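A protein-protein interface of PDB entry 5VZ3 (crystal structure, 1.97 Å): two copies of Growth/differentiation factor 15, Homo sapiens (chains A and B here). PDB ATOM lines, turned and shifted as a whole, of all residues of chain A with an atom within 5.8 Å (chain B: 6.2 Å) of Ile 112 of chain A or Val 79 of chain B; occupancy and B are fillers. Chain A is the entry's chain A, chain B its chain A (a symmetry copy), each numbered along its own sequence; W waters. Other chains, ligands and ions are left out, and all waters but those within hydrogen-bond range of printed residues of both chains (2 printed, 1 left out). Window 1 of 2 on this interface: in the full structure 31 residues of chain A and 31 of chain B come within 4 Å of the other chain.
Among the printed residues, pairs that only touch across the chains: His 58 of chain A with Pro 80 of chain B (3.9 Å), His 58 of chain A with Tyr 83 of chain B (3.7 Å), Val 79 of chain A with Ile 112 of chain B (3.6 Å), Ile 112 of chain A with Val 79 of chain B (3.6 Å) and Ile 112 of chain A with Tyr 83 of chain B (3.6 Å).
Cys 48 of chain A touches none of the printed residues of chain B. Of the printed residues of chain B, Asn 56 of chain A touches Tyr 83. Of the printed residues of chain B, His 58 of chain A touches Pro 80 and Tyr 83. Of the printed residues of chain B, Ile 112 of chain A touches Val 79 (3.6 Å) and Tyr 83 (3.6 Å). Printed residues of chain A within 4 Å of Ile 112 of chain B: Val 79 (3.6 Å). The nearest printed residue of chain A that does not touch Val 79 of chain B is Val 79 of chain A (4.01 Å).
Water W2 lies within hydrogen-bond range of the side-chain amino group of Lys 62 of chain A (2.5 Å), the backbone carbonyl oxygen of Cys 78 of chain B (2.7 Å) and the backbone carbonyl oxygen of Cys 44 of chain B (3.2 Å). Water W1 lies within hydrogen-bond range of a ring nitrogen (NE2) of His 58 of chain A (2.7 Å) and the backbone NH of Cys 44 of chain B (2.8 Å).
The side-chain sulfur of Cys 77 of chain A lies close to the side-chain sulfur of Cys 77 of chain B (3.0 Å). OH of Tyr 83 of chain B is in hydrogen-bond range of ND2 of Asn 56 of chain A (2.9 Å).
Cys 77 of chain A touches its own counterpart, Cys 77 of chain B. Val 79 of chain A touches Ile 112 of chain B, and with the chains exchanged Ile 112 of chain A touches Val 79 of chain B. 7 positions are printed for both chains.
Hydrophobic or aromatic side chains of chain B that line the printed part of chain A: Val 79, Pro 80, Tyr 83 and Ile 112. Printed residues of chain A that touch a printed residue of chain B: Asn 56, His 58, Cys 77, Val 79 and Ile 112. Hydrophobic or aromatic side chains of chain A within 4 Å of the printed part of chain B: His 58, Val 79 and Ile 112.
The backbone carbonyl oxygen (O) of Cys 77 of chain B is in hydrogen-bond range of the backbone NH (N) of Ile 112 of chain B, at 3.0 Å. SG of Cys 78 of chain B is disulfide-bonded to SG of Cys 15 of chain B (2.0 Å). The backbone carbonyl oxygen (O) of Cys 77 of chain A lies within hydrogen-bond range of the backbone NH (N) of Ile 112 of chain A. OD1 of Asn 56 of chain A is in hydrogen-bond range of N of Ala 59 of chain A (3.0 Å). The backbone NH (N) of Val 79 of chain A lies within hydrogen-bond range of the backbone carbonyl oxygen (O) of His 110 of chain A, at 2.9 Å. N of His 58 of chain A is in hydrogen-bond range of OD1 of Asn 56 of chain A (3.0 Å).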
ATOM      1  N   CYS A  48      14.766   0.982   1.811  1.00  0.00           N
ATOM      2  CA  CYS A  48      15.666   1.761   0.945  1.00  0.00           C
ATOM      3  C   CYS A  48      17.072   1.749   1.561  1.00  0.00           C
ATOM      4  O   CYS A  48      17.519   2.755   2.084  1.00  0.00           O
ATOM      5  CB  CYS A  48      15.164   3.210   0.828  1.00  0.00           C
ATOM      6  SG  CYS A  48      13.833   3.409  -0.386  1.00  0.00           S
ATOM      7  N   ARG A  53      18.535   1.764  -5.394  1.00  0.00           N
ATOM      8  CA  ARG A  53      17.707   2.601  -6.233  1.00  0.00           C
ATOM      9  C   ARG A  53      17.696   4.051  -5.786  1.00  0.00           C
ATOM     10  O   ARG A  53      16.599   4.653  -5.669  1.00  0.00           O
ATOM     11  CB  ARG A  53      16.251   2.107  -6.250  1.00  0.00           C
ATOM     12  CG  ARG A  53      16.038   0.802  -6.964  1.00  0.00           C
ATOM     13  CD  ARG A  53      14.629   0.705  -7.522  1.00  0.00           C
ATOM     14  NE  ARG A  53      14.113  -0.651  -7.410  1.00  0.00           N
ATOM     15  CZ  ARG A  53      12.901  -1.039  -7.804  1.00  0.00           C
ATOM     16  NH1 ARG A  53      12.045  -0.178  -8.368  1.00  0.00           N
ATOM     17  NH2 ARG A  53      12.546  -2.313  -7.630  1.00  0.00           N
ATOM     18  N   ALA A  55      17.455   7.683  -6.027  1.00  0.00           N
ATOM     19  CA  ALA A  55      16.948   8.534  -7.089  1.00  0.00           C
ATOM     20  C   ALA A  55      17.971   9.552  -7.546  1.00  0.00           C
ATOM     21  O   ALA A  55      17.961   9.930  -8.689  1.00  0.00           O
ATOM     22  CB  ALA A  55      15.738   9.282  -6.612  1.00  0.00           C
ATOM     23  N   ASN A  56      18.827  10.013  -6.637  1.00  0.00           N
ATOM     24  CA  ASN A  56      19.706  11.104  -6.914  1.00  0.00           C
ATOM     25  C   ASN A  56      20.694  11.251  -5.769  1.00  0.00           C
ATOM     26  O   ASN A  56      20.678  10.470  -4.801  1.00  0.00           O
ATOM     27  CB  ASN A  56      18.898  12.381  -7.136  1.00  0.00           C
ATOM     28  CG  ASN A  56      18.043  12.746  -5.960  1.00  0.00           C
ATOM     29  OD1 ASN A  56      18.355  12.452  -4.825  1.00  0.00           O
ATOM     30  ND2 ASN A  56      16.951  13.387  -6.230  1.00  0.00           N
ATOM     31  N   HIS A  58      20.852  13.570  -3.503  1.00  0.00           N
ATOM     32  CA  HIS A  58      20.194  13.903  -2.252  1.00  0.00           C
ATOM     33  C   HIS A  58      19.865  12.645  -1.429  1.00  0.00           C
ATOM     34  O   HIS A  58      19.983  12.644  -0.208  1.00  0.00           O
ATOM     35  CB  HIS A  58      18.941  14.694  -2.487  1.00  0.00           C
ATOM     36  CG  HIS A  58      18.320  15.226  -1.254  1.00  0.00           C
ATOM     37  ND1 HIS A  58      18.840  16.279  -0.561  1.00  0.00           N
ATOM     38  CD2 HIS A  58      17.207  14.845  -0.588  1.00  0.00           C
ATOM     39  CE1 HIS A  58      18.056  16.578   0.445  1.00  0.00           C
ATOM     40  NE2 HIS A  58      17.068  15.695   0.469  1.00  0.00           N
ATOM     41  N   ALA A  59      19.432  11.585  -2.113  1.00  0.00           N
ATOM     42  CA  ALA A  59      19.115  10.304  -1.472  1.00  0.00           C
ATOM     43  C   ALA A  59      20.315   9.682  -0.808  1.00  0.00           C
ATOM     44  O   ALA A  59      20.222   9.125   0.301  1.00  0.00           O
ATOM     45  CB  ALA A  59      18.556   9.352  -2.477  1.00  0.00           C
ATOM     46  N   LYS A  62      21.016  11.631   2.364  1.00  0.00           N
ATOM     47  CA  LYS A  62      20.109  11.159   3.396  1.00  0.00           C
ATOM     48  C   LYS A  62      20.493   9.815   4.007  1.00  0.00           C
ATOM     49  O   LYS A  62      20.382   9.638   5.191  1.00  0.00           O
ATOM     50  CB  LYS A  62      18.692  11.079   2.874  1.00  0.00           C
ATOM     51  CG  LYS A  62      18.054  12.433   2.849  1.00  0.00           C
ATOM     52  CD  LYS A  62      16.684  12.355   2.181  1.00  0.00           C
ATOM     53  CE  LYS A  62      15.604  11.877   3.131  1.00  0.00           C
ATOM     54  NZ  LYS A  62      14.380  11.505   2.322  1.00  0.00           N
ATOM     55  N   ALA A  75      15.758   7.924   6.998  1.00  0.00           N
ATOM     56  CA  ALA A  75      16.178   7.195   5.754  1.00  0.00           C
ATOM     57  C   ALA A  75      15.489   7.684   4.451  1.00  0.00           C
ATOM     58  O   ALA A  75      14.415   8.251   4.517  1.00  0.00           O
ATOM     59  CB  ALA A  75      15.881   5.731   5.933  1.00  0.00           C
ATOM     60  N   PRO A  76      16.094   7.450   3.274  1.00  0.00           N
ATOM     61  CA  PRO A  76      15.298   7.619   2.063  1.00  0.00           C
ATOM     62  C   PRO A  76      14.036   6.763   2.090  1.00  0.00           C
ATOM     63  O   PRO A  76      14.014   5.697   2.683  1.00  0.00           O
ATOM     64  CB  PRO A  76      16.241   7.180   0.940  1.00  0.00           C
ATOM     65  CG  PRO A  76      17.576   7.233   1.538  1.00  0.00           C
ATOM     66  CD  PRO A  76      17.436   6.936   2.971  1.00  0.00           C
ATOM     67  N   CYS A  77      12.999   7.261   1.425  1.00  0.00           N
ATOM     68  CA  CYS A  77      11.681   6.621   1.371  1.00  0.00           C
ATOM     69  C   CYS A  77      11.431   6.053  -0.021  1.00  0.00           C
ATOM     70  O   CYS A  77      11.839   6.654  -1.008  1.00  0.00           O
ATOM     71  CB  CYS A  77      10.597   7.674   1.656  1.00  0.00           C
ATOM     72  SG  CYS A  77       8.895   7.052   1.805  1.00  0.00           S
ATOM     73  N   CYS A  78      10.695   4.942  -0.091  1.00  0.00           N
ATOM     74  CA  CYS A  78      10.284   4.360  -1.378  1.00  0.00           C
ATOM     75  C   CYS A  78       9.070   5.125  -1.906  1.00  0.00           C
ATOM     76  O   CYS A  78       7.980   5.156  -1.279  1.00  0.00           O
ATOM     77  CB  CYS A  78       9.936   2.916  -1.095  1.00  0.00           C
ATOM     78  SG  CYS A  78       9.558   1.948  -2.535  1.00  0.00           S
ATOM     79  N   VAL A  79       9.238   5.780  -3.033  1.00  0.00           N
ATOM     80  CA  VAL A  79       8.209   6.591  -3.618  1.00  0.00           C
ATOM     81  C   VAL A  79       8.133   6.353  -5.167  1.00  0.00           C
ATOM     82  O   VAL A  79       9.059   5.911  -5.762  1.00  0.00           O
ATOM     83  CB  VAL A  79       8.410   8.087  -3.343  1.00  0.00           C
ATOM     84  CG1 VAL A  79       8.591   8.348  -1.847  1.00  0.00           C
ATOM     85  CG2 VAL A  79       9.612   8.625  -4.073  1.00  0.00           C
ATOM     86  N   HIS A 110      11.443   4.411  -6.668  1.00  0.00           N
ATOM     87  CA  HIS A 110      12.837   4.636  -6.306  1.00  0.00           C
ATOM     88  C   HIS A 110      12.897   5.276  -4.896  1.00  0.00           C
ATOM     89  O   HIS A 110      11.861   5.616  -4.313  1.00  0.00           O
ATOM     90  CB  HIS A 110      13.529   5.479  -7.386  1.00  0.00           C
ATOM     91  CG  HIS A 110      12.950   6.822  -7.586  1.00  0.00           C
ATOM     92  ND1 HIS A 110      13.423   7.678  -8.545  1.00  0.00           N
ATOM     93  CD2 HIS A 110      11.950   7.486  -6.955  1.00  0.00           C
ATOM     94  CE1 HIS A 110      12.768   8.819  -8.471  1.00  0.00           C
ATOM     95  NE2 HIS A 110      11.867   8.726  -7.516  1.00  0.00           N
ATOM     96  N   CYS A 111      14.102   5.318  -4.338  1.00  0.00           N
ATOM     97  CA  CYS A 111      14.391   5.755  -2.971  1.00  0.00           C
ATOM     98  C   CYS A 111      14.846   7.196  -3.001  1.00  0.00           C
ATOM     99  O   CYS A 111      15.825   7.534  -3.682  1.00  0.00           O
ATOM    100  CB  CYS A 111      15.465   4.887  -2.388  1.00  0.00           C
ATOM    101  SG  CYS A 111      14.830   3.180  -2.192  1.00  0.00           S
ATOM    102  N   ILE A 112      14.146   8.072  -2.300  1.00  0.00           N
ATOM    103  CA  ILE A 112      14.409   9.511  -2.461  1.00  0.00           C
ATOM    104  C   ILE A 112      14.500  10.277  -1.160  1.00  0.00           C
ATOM    105  O   ILE A 112      14.006   9.746  -0.117  1.00  0.00           O
ATOM    106  CB  ILE A 112      13.317  10.121  -3.336  1.00  0.00           C
ATOM    107  CG1 ILE A 112      13.860  11.243  -4.246  1.00  0.00           C
ATOM    108  CG2 ILE A 112      12.168  10.591  -2.476  1.00  0.00           C
ATOM    109  CD1 ILE A 112      13.187  11.261  -5.623  1.00  0.00           C
ATOM    110  OXT ILE A 112      15.014  11.443  -1.219  1.00  0.00           O
ATOM    111  N   CYS B  15       5.863  17.831   7.754  1.00  0.00           N
ATOM    112  CA  CYS B  15       6.711  17.857   6.632  1.00  0.00           C
ATOM    113  C   CYS B  15       7.094  19.264   6.230  1.00  0.00           C
ATOM    114  O   CYS B  15       6.223  20.059   5.813  1.00  0.00           O
ATOM    115  CB  CYS B  15       5.999  17.183   5.484  1.00  0.00           C
ATOM    116  SG  CYS B  15       6.949  17.118   3.966  1.00  0.00           S
ATOM    117  N   CYS B  44      13.892  17.623   3.557  1.00  0.00           N
ATOM    118  CA  CYS B  44      12.493  17.587   3.880  1.00  0.00           C
ATOM    119  C   CYS B  44      12.334  16.580   4.962  1.00  0.00           C
ATOM    120  O   CYS B  44      12.663  15.408   4.813  1.00  0.00           O
ATOM    121  CB  CYS B  44      11.683  17.160   2.657  1.00  0.00           C
ATOM    122  SG  CYS B  44      11.758  18.390   1.341  1.00  0.00           S
ATOM    123  N   CYS B  48       3.502  13.451   7.880  1.00  0.00           N
ATOM    124  CA  CYS B  48       2.607  13.659   6.729  1.00  0.00           C
ATOM    125  C   CYS B  48       1.199  13.183   7.110  1.00  0.00           C
ATOM    126  O   CYS B  48       0.751  12.154   6.634  1.00  0.00           O
ATOM    127  CB  CYS B  48       3.114  12.861   5.516  1.00  0.00           C
ATOM    128  SG  CYS B  48       4.451  13.695   4.620  1.00  0.00           S
ATOM    129  N   CYS B  77       5.285   9.899   2.693  1.00  0.00           N
ATOM    130  CA  CYS B  77       6.602  10.331   3.172  1.00  0.00           C
ATOM    131  C   CYS B  77       6.857  11.779   2.768  1.00  0.00           C
ATOM    132  O   CYS B  77       6.456  12.191   1.686  1.00  0.00           O
ATOM    133  CB  CYS B  77       7.687   9.458   2.521  1.00  0.00           C
ATOM    134  SG  CYS B  77       9.387   9.717   3.111  1.00  0.00           S
ATOM    135  N   CYS B  78       7.591  12.514   3.605  1.00  0.00           N
ATOM    136  CA  CYS B  78       8.007  13.886   3.277  1.00  0.00           C
ATOM    137  C   CYS B  78       9.225  13.831   2.355  1.00  0.00           C
ATOM    138  O   CYS B  78      10.312  13.314   2.720  1.00  0.00           O
ATOM    139  CB  CYS B  78       8.350  14.548   4.593  1.00  0.00           C
ATOM    140  SG  CYS B  78       8.733  16.278   4.476  1.00  0.00           S
ATOM    141  N   VAL B  79       9.064  14.320   1.145  1.00  0.00           N
ATOM    142  CA  VAL B  79      10.097  14.282   0.151  1.00  0.00           C
ATOM    143  C   VAL B  79      10.180  15.650  -0.611  1.00  0.00           C
ATOM    144  O   VAL B  79       9.256  16.394  -0.631  1.00  0.00           O
ATOM    145  CB  VAL B  79       9.899  13.146  -0.863  1.00  0.00           C
ATOM    146  CG1 VAL B  79       9.711  11.806  -0.151  1.00  0.00           C
ATOM    147  CG2 VAL B  79       8.701  13.396  -1.741  1.00  0.00           C
ATOM    148  N   PRO B  80      11.305  15.919  -1.225  1.00  0.00           N
ATOM    149  CA  PRO B  80      11.493  17.169  -1.913  1.00  0.00           C
ATOM    150  C   PRO B  80      10.540  17.223  -3.111  1.00  0.00           C
ATOM    151  O   PRO B  80      10.380  16.251  -3.843  1.00  0.00           O
ATOM    152  CB  PRO B  80      12.940  17.096  -2.389  1.00  0.00           C
ATOM    153  CG  PRO B  80      13.588  16.048  -1.600  1.00  0.00           C
ATOM    154  CD  PRO B  80      12.489  15.054  -1.316  1.00  0.00           C
ATOM    155  N   ALA B  81       9.862  18.329  -3.240  1.00  0.00           N
ATOM    156  CA  ALA B  81       9.114  18.627  -4.455  1.00  0.00           C
ATOM    157  C   ALA B  81      10.025  19.241  -5.493  1.00  0.00           C
ATOM    158  O   ALA B  81       9.765  19.134  -6.669  1.00  0.00           O
ATOM    159  CB  ALA B  81       7.968  19.557  -4.139  1.00  0.00           C
ATOM    160  N   SER B  82      11.119  19.848  -5.072  1.00  0.00           N
ATOM    161  CA  SER B  82      12.057  20.449  -6.015  1.00  0.00           C
ATOM    162  C   SER B  82      13.386  20.580  -5.315  1.00  0.00           C
ATOM    163  O   SER B  82      13.463  20.490  -4.087  1.00  0.00           O
ATOM    164  CB  SER B  82      11.575  21.848  -6.486  1.00  0.00           C
ATOM    165  OG  SER B  82      11.416  22.723  -5.412  1.00  0.00           O
ATOM    166  N   TYR B  83      14.410  20.841  -6.108  1.00  0.00           N
ATOM    167  CA  TYR B  83      15.785  21.044  -5.628  1.00  0.00           C
ATOM    168  C   TYR B  83      16.419  22.460  -5.910  1.00  0.00           C
ATOM    169  O   TYR B  83      15.948  23.258  -6.748  1.00  0.00           O
ATOM    170  CB  TYR B  83      16.659  19.909  -6.203  1.00  0.00           C
ATOM    171  CG  TYR B  83      16.200  18.524  -5.791  1.00  0.00           C
ATOM    172  CD1 TYR B  83      15.233  17.864  -6.516  1.00  0.00           C
ATOM    173  CD2 TYR B  83      16.742  17.872  -4.686  1.00  0.00           C
ATOM    174  CE1 TYR B  83      14.795  16.606  -6.151  1.00  0.00           C
ATOM    175  CE2 TYR B  83      16.309  16.585  -4.307  1.00  0.00           C
ATOM    176  CZ  TYR B  83      15.337  15.961  -5.037  1.00  0.00           C
ATOM    177  OH  TYR B  83      14.868  14.704  -4.706  1.00  0.00           O
ATOM    178  N   ASP B 108      11.822  22.683  -1.755  1.00  0.00           N
ATOM    179  CA  ASP B 108      10.558  22.612  -1.041  1.00  0.00           C
ATOM    180  C   ASP B 108      10.166  21.116  -0.900  1.00  0.00           C
ATOM    181  O   ASP B 108      10.804  20.251  -1.541  1.00  0.00           O
ATOM    182  CB  ASP B 108       9.474  23.435  -1.777  1.00  0.00           C
ATOM    183  CG  ASP B 108       9.289  23.006  -3.231  1.00  0.00           C
ATOM    184  OD1 ASP B 108      10.073  22.144  -3.735  1.00  0.00           O
ATOM    185  OD2 ASP B 108       8.365  23.548  -3.890  1.00  0.00           O
ATOM    186  N   CYS B 109       9.104  20.889  -0.119  1.00  0.00           N
ATOM    187  CA  CYS B 109       8.694  19.576   0.406  1.00  0.00           C
ATOM    188  C   CYS B 109       7.201  19.293   0.193  1.00  0.00           C
ATOM    189  O   CYS B 109       6.354  20.171   0.283  1.00  0.00           O
ATOM    190  CB  CYS B 109       8.987  19.565   1.895  1.00  0.00           C
ATOM    191  SG  CYS B 109      10.739  19.999   2.222  1.00  0.00           S
ATOM    192  N   HIS B 110       6.873  18.035  -0.014  1.00  0.00           N
ATOM    193  CA  HIS B 110       5.478  17.614   0.024  1.00  0.00           C
ATOM    194  C   HIS B 110       5.413  16.109   0.384  1.00  0.00           C
ATOM    195  O   HIS B 110       6.446  15.437   0.478  1.00  0.00           O
ATOM    196  CB  HIS B 110       4.793  17.951  -1.307  1.00  0.00           C
ATOM    197  CG  HIS B 110       5.376  17.284  -2.488  1.00  0.00           C
ATOM    198  ND1 HIS B 110       4.909  17.517  -3.755  1.00  0.00           N
ATOM    199  CD2 HIS B 110       6.374  16.376  -2.620  1.00  0.00           C
ATOM    200  CE1 HIS B 110       5.567  16.757  -4.607  1.00  0.00           C
ATOM    201  NE2 HIS B 110       6.463  16.058  -3.943  1.00  0.00           N
ATOM    202  N   CYS B 111       4.206  15.645   0.687  1.00  0.00           N
ATOM    203  CA  CYS B 111       3.911  14.298   1.180  1.00  0.00           C
ATOM    204  C   CYS B 111       3.459  13.438   0.021  1.00  0.00           C
ATOM    205  O   CYS B 111       2.484  13.771  -0.669  1.00  0.00           O
ATOM    206  CB  CYS B 111       2.831  14.372   2.217  1.00  0.00           C
ATOM    207  SG  CYS B 111       3.462  15.263   3.688  1.00  0.00           S
ATOM    208  N   ILE B 112       4.158  12.346  -0.238  1.00  0.00           N
ATOM    209  CA  ILE B 112       3.899  11.591  -1.474  1.00  0.00           C
ATOM    210  C   ILE B 112       3.804  10.093  -1.281  1.00  0.00           C
ATOM    211  O   ILE B 112       4.291   9.595  -0.219  1.00  0.00           O
ATOM    212  CB  ILE B 112       4.997  11.905  -2.488  1.00  0.00           C
ATOM    213  CG1 ILE B 112       4.460  11.937  -3.934  1.00  0.00           C
ATOM    214  CG2 ILE B 112       6.143  10.935  -2.325  1.00  0.00           C
ATOM    215  CD1 ILE B 112       5.140  13.011  -4.790  1.00  0.00           C
ATOM    216  OXT ILE B 112       3.292   9.427  -2.240  1.00  0.00           O
HETATM  217  O   HOH W   1      14.702  15.740   1.710  1.00  0.00           O
HETATM  218  O   HOH W   2      12.916  13.575   2.227  1.00  0.00           O
